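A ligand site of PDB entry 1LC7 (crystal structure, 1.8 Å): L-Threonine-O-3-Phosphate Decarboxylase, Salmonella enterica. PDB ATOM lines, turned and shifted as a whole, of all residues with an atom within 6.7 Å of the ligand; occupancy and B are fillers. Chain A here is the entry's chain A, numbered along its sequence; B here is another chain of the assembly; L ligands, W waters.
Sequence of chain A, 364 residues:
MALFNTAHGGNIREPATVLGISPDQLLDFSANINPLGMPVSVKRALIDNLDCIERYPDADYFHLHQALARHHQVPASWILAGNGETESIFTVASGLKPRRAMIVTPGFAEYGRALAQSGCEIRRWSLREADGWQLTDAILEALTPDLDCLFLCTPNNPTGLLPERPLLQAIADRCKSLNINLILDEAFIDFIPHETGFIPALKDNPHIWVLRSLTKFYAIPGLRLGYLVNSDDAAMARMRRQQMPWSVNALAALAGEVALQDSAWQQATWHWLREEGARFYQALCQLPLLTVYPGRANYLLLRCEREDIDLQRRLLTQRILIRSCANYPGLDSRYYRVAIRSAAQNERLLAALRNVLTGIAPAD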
ATOM      1  N   ALA A   7      -7.872   2.629  -0.804  1.00  0.00           N
ATOM      2  CA  ALA A   7      -9.062   2.139  -1.514  1.00  0.00           C
ATOM      3  C   ALA A   7      -9.614   3.230  -2.455  1.00  0.00           C
ATOM      4  O   ALA A   7     -10.262   2.918  -3.455  1.00  0.00           O
ATOM      5  CB  ALA A   7     -10.141   1.724  -0.491  1.00  0.00           C
ATOM      6  N   HIS A   8      -9.376   4.499  -2.111  1.00  0.00           N
ATOM      7  CA  HIS A   8      -9.850   5.604  -2.967  1.00  0.00           C
ATOM      8  C   HIS A   8      -8.802   6.715  -3.132  1.00  0.00           C
ATOM      9  O   HIS A   8      -7.912   6.881  -2.289  1.00  0.00           O
ATOM     10  CB  HIS A   8     -11.150   6.217  -2.410  1.00  0.00           C
ATOM     11  CG  HIS A   8     -12.293   5.249  -2.335  1.00  0.00           C
ATOM     12  ND1 HIS A   8     -12.836   4.658  -3.453  1.00  0.00           N
ATOM     13  CD2 HIS A   8     -12.973   4.757  -1.273  1.00  0.00           C
ATOM     14  CE1 HIS A   8     -13.806   3.838  -3.088  1.00  0.00           C
ATOM     15  NE2 HIS A   8     -13.914   3.886  -1.767  1.00  0.00           N
ATOM     16  N   GLY A   9      -8.932   7.456  -4.231  1.00  0.00           N
ATOM     17  CA  GLY A   9      -8.039   8.581  -4.502  1.00  0.00           C
ATOM     18  C   GLY A   9      -8.378   9.733  -3.574  1.00  0.00           C
ATOM     19  O   GLY A   9      -9.227   9.594  -2.684  1.00  0.00           O
ATOM     20  N   GLY A  10      -7.710  10.876  -3.771  1.00  0.00           N
ATOM     21  CA  GLY A  10      -7.934  12.043  -2.954  1.00  0.00           C
ATOM     22  C   GLY A  10      -7.277  11.965  -1.578  1.00  0.00           C
ATOM     23  O   GLY A  10      -7.466  12.868  -0.743  1.00  0.00           O
ATOM     24  N   SER A  30      -5.441  12.802  -8.125  1.00  0.00           N
ATOM     25  CA  SER A  30      -6.033  11.489  -7.818  1.00  0.00           C
ATOM     26  C   SER A  30      -7.531  11.449  -7.529  1.00  0.00           C
ATOM     27  O   SER A  30      -8.094  10.365  -7.396  1.00  0.00           O
ATOM     28  CB  SER A  30      -5.267  10.824  -6.658  1.00  0.00           C
ATOM     29  OG  SER A  30      -5.590  11.471  -5.440  1.00  0.00           O
ATOM     30  N   ALA A  31      -8.156  12.620  -7.397  1.00  0.00           N
ATOM     31  CA  ALA A  31      -9.595  12.742  -7.168  1.00  0.00           C
ATOM     32  C   ALA A  31     -10.053  13.637  -8.314  1.00  0.00           C
ATOM     33  O   ALA A  31      -9.303  14.515  -8.731  1.00  0.00           O
ATOM     34  CB  ALA A  31      -9.888  13.424  -5.813  1.00  0.00           C
ATOM     35  N   ASN A  32     -11.270  13.451  -8.786  1.00  0.00           N
ATOM     36  CA  ASN A  32     -11.748  14.197  -9.951  1.00  0.00           C
ATOM     37  C   ASN A  32     -12.777  15.232  -9.672  1.00  0.00           C
ATOM     38  O   ASN A  32     -13.968  15.072  -9.992  1.00  0.00           O
ATOM     39  CB  ASN A  32     -12.276  13.163 -10.922  1.00  0.00           C
ATOM     40  CG  ASN A  32     -11.285  12.075 -11.127  1.00  0.00           C
ATOM     41  OD1 ASN A  32     -10.138  12.356 -11.417  1.00  0.00           O
ATOM     42  ND2 ASN A  32     -11.711  10.818 -10.979  1.00  0.00           N
ATOM     43  N   ILE A  33     -12.318  16.320  -9.072  1.00  0.00           N
ATOM     44  CA  ILE A  33     -13.198  17.415  -8.686  1.00  0.00           C
ATOM     45  C   ILE A  33     -13.096  18.557  -9.683  1.00  0.00           C
ATOM     46  O   ILE A  33     -11.989  18.907 -10.104  1.00  0.00           O
ATOM     47  CB  ILE A  33     -12.799  17.946  -7.272  1.00  0.00           C
ATOM     48  CG1 ILE A  33     -12.662  16.783  -6.264  1.00  0.00           C
ATOM     49  CG2 ILE A  33     -13.855  18.916  -6.777  1.00  0.00           C
ATOM     50  CD1 ILE A  33     -13.930  15.976  -6.120  1.00  0.00           C
ATOM     51  N   PHE A 108     -15.907   1.216  -9.871  1.00  0.00           N
ATOM     52  CA  PHE A 108     -15.830   1.828  -8.529  1.00  0.00           C
ATOM     53  C   PHE A 108     -15.910   0.692  -7.497  1.00  0.00           C
ATOM     54  O   PHE A 108     -16.789  -0.150  -7.582  1.00  0.00           O
ATOM     55  CB  PHE A 108     -17.004   2.791  -8.385  1.00  0.00           C
ATOM     56  CG  PHE A 108     -16.930   3.649  -7.196  1.00  0.00           C
ATOM     57  CD1 PHE A 108     -15.732   4.278  -6.857  1.00  0.00           C
ATOM     58  CD2 PHE A 108     -18.061   3.848  -6.405  1.00  0.00           C
ATOM     59  CE1 PHE A 108     -15.666   5.097  -5.727  1.00  0.00           C
ATOM     60  CE2 PHE A 108     -18.000   4.667  -5.283  1.00  0.00           C
ATOM     61  CZ  PHE A 108     -16.807   5.287  -4.931  1.00  0.00           C
ATOM     62  N   ALA A 109     -15.005   0.671  -6.500  1.00  0.00           N
ATOM     63  CA  ALA A 109     -14.980  -0.427  -5.524  1.00  0.00           C
ATOM     64  C   ALA A 109     -16.179  -0.582  -4.598  1.00  0.00           C
ATOM     65  O   ALA A 109     -16.465  -1.684  -4.116  1.00  0.00           O
ATOM     66  CB  ALA A 109     -13.712  -0.333  -4.676  1.00  0.00           C
ATOM     67  N   ASN A 157     -15.745   4.289 -14.217  1.00  0.00           N
ATOM     68  CA  ASN A 157     -14.592   4.746 -13.478  1.00  0.00           C
ATOM     69  C   ASN A 157     -13.787   3.454 -13.265  1.00  0.00           C
ATOM     70  O   ASN A 157     -14.318   2.457 -12.757  1.00  0.00           O
ATOM     71  CB  ASN A 157     -14.997   5.350 -12.161  1.00  0.00           C
ATOM     72  CG  ASN A 157     -13.811   5.902 -11.442  1.00  0.00           C
ATOM     73  OD1 ASN A 157     -13.636   7.113 -11.359  1.00  0.00           O
ATOM     74  ND2 ASN A 157     -12.950   5.008 -10.968  1.00  0.00           N
ATOM     75  N   PRO A 158     -12.482   3.475 -13.572  1.00  0.00           N
ATOM     76  CA  PRO A 158     -11.616   4.543 -14.044  1.00  0.00           C
ATOM     77  C   PRO A 158     -11.403   4.799 -15.539  1.00  0.00           C
ATOM     78  O   PRO A 158     -10.627   5.693 -15.900  1.00  0.00           O
ATOM     79  CB  PRO A 158     -10.291   4.163 -13.403  1.00  0.00           C
ATOM     80  CG  PRO A 158     -10.259   2.702 -13.740  1.00  0.00           C
ATOM     81  CD  PRO A 158     -11.689   2.217 -13.511  1.00  0.00           C
ATOM     82  N   PHE A 188     -20.602  10.925 -13.054  1.00  0.00           N
ATOM     83  CA  PHE A 188     -19.908  11.896 -13.914  1.00  0.00           C
ATOM     84  C   PHE A 188     -20.639  12.318 -15.182  1.00  0.00           C
ATOM     85  O   PHE A 188     -20.062  13.019 -16.020  1.00  0.00           O
ATOM     86  CB  PHE A 188     -18.550  11.321 -14.349  1.00  0.00           C
ATOM     87  CG  PHE A 188     -17.583  11.164 -13.219  1.00  0.00           C
ATOM     88  CD1 PHE A 188     -17.437   9.947 -12.571  1.00  0.00           C
ATOM     89  CD2 PHE A 188     -16.841  12.252 -12.781  1.00  0.00           C
ATOM     90  CE1 PHE A 188     -16.591   9.806 -11.509  1.00  0.00           C
ATOM     91  CE2 PHE A 188     -15.981  12.129 -11.702  1.00  0.00           C
ATOM     92  CZ  PHE A 188     -15.850  10.904 -11.057  1.00  0.00           C
ATOM     93  N   LYS A 216     -18.598  16.082  -7.377  1.00  0.00           N
ATOM     94  CA  LYS A 216     -17.561  16.293  -8.377  1.00  0.00           C
ATOM     95  C   LYS A 216     -17.867  17.493  -9.284  1.00  0.00           C
ATOM     96  O   LYS A 216     -17.042  18.408  -9.414  1.00  0.00           O
ATOM     97  CB  LYS A 216     -17.391  15.035  -9.210  1.00  0.00           C
ATOM     98  CG  LYS A 216     -17.168  13.801  -8.330  1.00  0.00           C
ATOM     99  CD  LYS A 216     -18.103  12.643  -8.688  1.00  0.00           C
ATOM    100  CE  LYS A 216     -17.916  11.479  -7.697  1.00  0.00           C
ATOM    101  NZ  LYS A 216     -16.473  11.133  -7.561  1.00  0.00           N
ATOM    102  N   TYR A 299     -11.532  13.045 -16.308  1.00  0.00           N
ATOM    103  CA  TYR A 299     -10.417  12.198 -15.882  1.00  0.00           C
ATOM    104  C   TYR A 299     -10.044  11.274 -17.035  1.00  0.00           C
ATOM    105  O   TYR A 299     -10.840  11.056 -17.961  1.00  0.00           O
ATOM    106  CB  TYR A 299     -10.781  11.371 -14.626  1.00  0.00           C
ATOM    107  CG  TYR A 299     -12.002  10.501 -14.796  1.00  0.00           C
ATOM    108  CD1 TYR A 299     -13.264  11.024 -14.538  1.00  0.00           C
ATOM    109  CD2 TYR A 299     -11.890   9.175 -15.209  1.00  0.00           C
ATOM    110  CE1 TYR A 299     -14.403  10.249 -14.686  1.00  0.00           C
ATOM    111  CE2 TYR A 299     -13.038   8.382 -15.365  1.00  0.00           C
ATOM    112  CZ  TYR A 299     -14.276   8.930 -15.095  1.00  0.00           C
ATOM    113  OH  TYR A 299     -15.451   8.224 -15.248  1.00  0.00           O
ATOM    114  N   ARG A 323      -3.706   8.703  -9.186  1.00  0.00           N
ATOM    115  CA  ARG A 323      -4.361   7.476  -8.739  1.00  0.00           C
ATOM    116  C   ARG A 323      -3.718   6.228  -9.344  1.00  0.00           C
ATOM    117  O   ARG A 323      -3.477   6.182 -10.544  1.00  0.00           O
ATOM    118  CB  ARG A 323      -5.855   7.546  -9.135  1.00  0.00           C
ATOM    119  CG  ARG A 323      -6.707   6.301  -8.752  1.00  0.00           C
ATOM    120  CD  ARG A 323      -6.893   6.162  -7.235  1.00  0.00           C
ATOM    121  NE  ARG A 323      -8.114   5.396  -6.950  1.00  0.00           N
ATOM    122  CZ  ARG A 323      -8.150   4.136  -6.528  1.00  0.00           C
ATOM    123  NH1 ARG A 323      -7.029   3.451  -6.329  1.00  0.00           N
ATOM    124  NH2 ARG A 323      -9.323   3.543  -6.285  1.00  0.00           N
ATOM    125  N   ASN A 327      -5.064  -1.713  -7.863  1.00  0.00           N
ATOM    126  CA  ASN A 327      -6.004  -2.365  -6.937  1.00  0.00           C
ATOM    127  C   ASN A 327      -7.370  -2.661  -7.557  1.00  0.00           C
ATOM    128  O   ASN A 327      -8.210  -3.305  -6.920  1.00  0.00           O
ATOM    129  CB  ASN A 327      -6.182  -1.472  -5.704  1.00  0.00           C
ATOM    130  CG  ASN A 327      -6.563  -0.039  -6.074  1.00  0.00           C
ATOM    131  OD1 ASN A 327      -7.710   0.397  -5.848  1.00  0.00           O
ATOM    132  ND2 ASN A 327      -5.607   0.692  -6.686  1.00  0.00           N
ATOM    133  N   TYR A 328      -7.631  -2.168  -8.761  1.00  0.00           N
ATOM    134  CA  TYR A 328      -8.895  -2.426  -9.423  1.00  0.00           C
ATOM    135  C   TYR A 328      -8.862  -3.817 -10.042  1.00  0.00           C
ATOM    136  O   TYR A 328      -7.949  -4.152 -10.771  1.00  0.00           O
ATOM    137  CB  TYR A 328      -9.101  -1.463 -10.591  1.00  0.00           C
ATOM    138  CG  TYR A 328      -9.586  -0.076 -10.187  1.00  0.00           C
ATOM    139  CD1 TYR A 328     -10.924   0.248 -10.201  1.00  0.00           C
ATOM    140  CD2 TYR A 328      -8.671   0.892  -9.794  1.00  0.00           C
ATOM    141  CE1 TYR A 328     -11.353   1.530  -9.843  1.00  0.00           C
ATOM    142  CE2 TYR A 328      -9.067   2.157  -9.434  1.00  0.00           C
ATOM    143  CZ  TYR A 328     -10.407   2.481  -9.470  1.00  0.00           C
ATOM    144  OH  TYR A 328     -10.800   3.776  -9.177  1.00  0.00           O
ATOM    145  N   ARG A 337      -4.699   6.749 -13.055  1.00  0.00           N
ATOM    146  CA  ARG A 337      -5.763   7.646 -13.493  1.00  0.00           C
ATOM    147  C   ARG A 337      -5.389   9.060 -13.035  1.00  0.00           C
ATOM    148  O   ARG A 337      -4.898   9.263 -11.901  1.00  0.00           O
ATOM    149  CB  ARG A 337      -7.107   7.307 -12.819  1.00  0.00           C
ATOM    150  CG  ARG A 337      -8.322   8.062 -13.396  1.00  0.00           C
ATOM    151  CD  ARG A 337      -9.567   7.815 -12.513  1.00  0.00           C
ATOM    152  NE  ARG A 337      -9.377   8.403 -11.192  1.00  0.00           N
ATOM    153  CZ  ARG A 337      -9.965   7.982 -10.081  1.00  0.00           C
ATOM    154  NH1 ARG A 337     -10.822   6.961 -10.143  1.00  0.00           N
ATOM    155  NH2 ARG A 337      -9.648   8.530  -8.908  1.00  0.00           N
ATOM    156  N   TYR B  56     -12.298  16.209  -0.719  1.00  0.00           N
ATOM    157  CA  TYR B  56     -12.921  15.160   0.091  1.00  0.00           C
ATOM    158  C   TYR B  56     -12.343  15.273   1.501  1.00  0.00           C
ATOM    159  O   TYR B  56     -11.257  15.794   1.694  1.00  0.00           O
ATOM    160  CB  TYR B  56     -12.521  13.751  -0.405  1.00  0.00           C
ATOM    161  CG  TYR B  56     -13.365  13.164  -1.512  1.00  0.00           C
ATOM    162  CD1 TYR B  56     -13.056  13.369  -2.848  1.00  0.00           C
ATOM    163  CD2 TYR B  56     -14.506  12.422  -1.201  1.00  0.00           C
ATOM    164  CE1 TYR B  56     -13.879  12.849  -3.865  1.00  0.00           C
ATOM    165  CE2 TYR B  56     -15.339  11.915  -2.200  1.00  0.00           C
ATOM    166  CZ  TYR B  56     -15.020  12.138  -3.528  1.00  0.00           C
ATOM    167  OH  TYR B  56     -15.900  11.652  -4.474  1.00  0.00           O
ATOM    168  N   TRP B 246     -15.769   8.251   3.968  1.00  0.00           N
ATOM    169  CA  TRP B 246     -16.060   9.676   4.067  1.00  0.00           C
ATOM    170  C   TRP B 246     -17.406   9.983   4.659  1.00  0.00           C
ATOM    171  O   TRP B 246     -18.108  10.872   4.174  1.00  0.00           O
ATOM    172  CB  TRP B 246     -16.024  10.309   2.673  1.00  0.00           C
ATOM    173  CG  TRP B 246     -14.818  10.002   1.849  1.00  0.00           C
ATOM    174  CD1 TRP B 246     -13.532  10.417   2.076  1.00  0.00           C
ATOM    175  CD2 TRP B 246     -14.830   9.376   0.560  1.00  0.00           C
ATOM    176  NE1 TRP B 246     -12.734  10.096   0.974  1.00  0.00           N
ATOM    177  CE2 TRP B 246     -13.511   9.444   0.042  1.00  0.00           C
ATOM    178  CE3 TRP B 246     -15.832   8.753  -0.204  1.00  0.00           C
ATOM    179  CZ2 TRP B 246     -13.166   8.924  -1.207  1.00  0.00           C
ATOM    180  CZ3 TRP B 246     -15.492   8.235  -1.462  1.00  0.00           C
ATOM    181  CH2 TRP B 246     -14.171   8.323  -1.944  1.00  0.00           C
HETATM  182  N1  LIG L   1     -14.620   8.232  -6.953  1.00  0.00           N
HETATM  183  C1  LIG L   1     -13.809   9.407  -6.649  1.00  0.00           C
HETATM  184  C2  LIG L   1     -12.476   8.871  -6.055  1.00  0.00           C
HETATM  185  C3  LIG L   1     -12.095   9.621  -4.790  1.00  0.00           C
HETATM  186  O1  LIG L   1     -12.611   7.530  -5.690  1.00  0.00           O
HETATM  187  P1  LIG L   1     -11.834   6.456  -6.629  1.00  0.00           P
HETATM  188  O2  LIG L   1     -12.015   5.045  -5.920  1.00  0.00           O
HETATM  189  O3  LIG L   1     -10.306   6.920  -6.708  1.00  0.00           O
HETATM  190  O4  LIG L   1     -12.578   6.513  -8.003  1.00  0.00           O
HETATM  191  C4  LIG L   1     -13.459  10.186  -7.892  1.00  0.00           C
HETATM  192  O5  LIG L   1     -12.889  11.321  -7.756  1.00  0.00           O
HETATM  193  O6  LIG L   1     -13.700   9.713  -9.065  1.00  0.00           O
HETATM  194  O   HOH W   1     -12.782   2.365  -6.586  1.00  0.00           O
HETATM  195  O   HOH W   2     -17.068   7.277  -8.911  1.00  0.00           O
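O2 of the ligand is in hydrogen-bond range of ND1 of His 8. An oxygen (O3) of the ligand lies within salt-bridge range of the guanidinium group of Arg 323 (2.7 Å). The guanidinium group (NH2) of Arg 337 lies within salt-bridge range of an oxygen (O3) of the ligand (2.8 Å). The backbone NH (N) of Asn 32 lies within hydrogen-bond range of an oxygen (O5) of the ligand. ND2 of Asn 32 is in hydrogen-bond range of O6 of the ligand, at 3.0 Å. O3 of the ligand is in hydrogen-bond range of N of Gly 9 (2.9 Å). The side-chain amino group (NZ) of Lys 216 lies within salt-bridge range of an oxygen (O6) of the ligand (3.5 Å). An oxygen (O4) of the ligand is in hydrogen-bond range of the side-chain amide nitrogen (ND2) of Asn 157 (3.3 Å). OH of Tyr 328 sits at hydrogen-bond distance from O4 of the ligand (3.5 Å).
The backbone carbonyl oxygen (O) of Arg 323 is in hydrogen-bond range of the backbone NH (N) of Arg 337 (2.8 Å). The backbone carbonyl oxygen (O) of Ala 7 lies within hydrogen-bond range of the guanidinium group (NH2) of Arg 323, 3.0 Å away. NH1 of Arg 323 sits close to ND2 of Asn 327 (3.1 Å). The guanidinium group of Arg 337 sits close to the side-chain amide nitrogen of Asn 32 (3.4 Å). The side-chain amide nitrogen (ND2) of Asn 157 lies close to the guanidinium group (NH1) of Arg 337. OH of Tyr 328 is in hydrogen-bond range of NH1 of Arg 337. The backbone carbonyl oxygen (O) of Ser 30 lies within hydrogen-bond range of the guanidinium group (NH2) of Arg 337 (2.8 Å). The side-chain amino group of Lys 216 lies within hydrogen-bond range of the side-chain hydroxyl of Tyr 56 of chain B.
Ala 7 touches the ligand. CA of Ala 31 touches O5 of the ligand (3.6 Å). Phe 108 touches the ligand. Phe 188 touches the ligand (CZ to O6, 3.2 Å). Tyr 56 of chain B touches the ligand (OH to C1, 3.8 Å). Trp 246 of chain B touches the ligand. Of the 21 residues printed, 14 come within 4 Å of the ligand. The nearest printed residue that does not touch the ligand is Ser 30 (4.2 Å).
Water W1 bridges N of Ala 109 (2.8 Å) and O2 of the ligand (2.9 Å).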
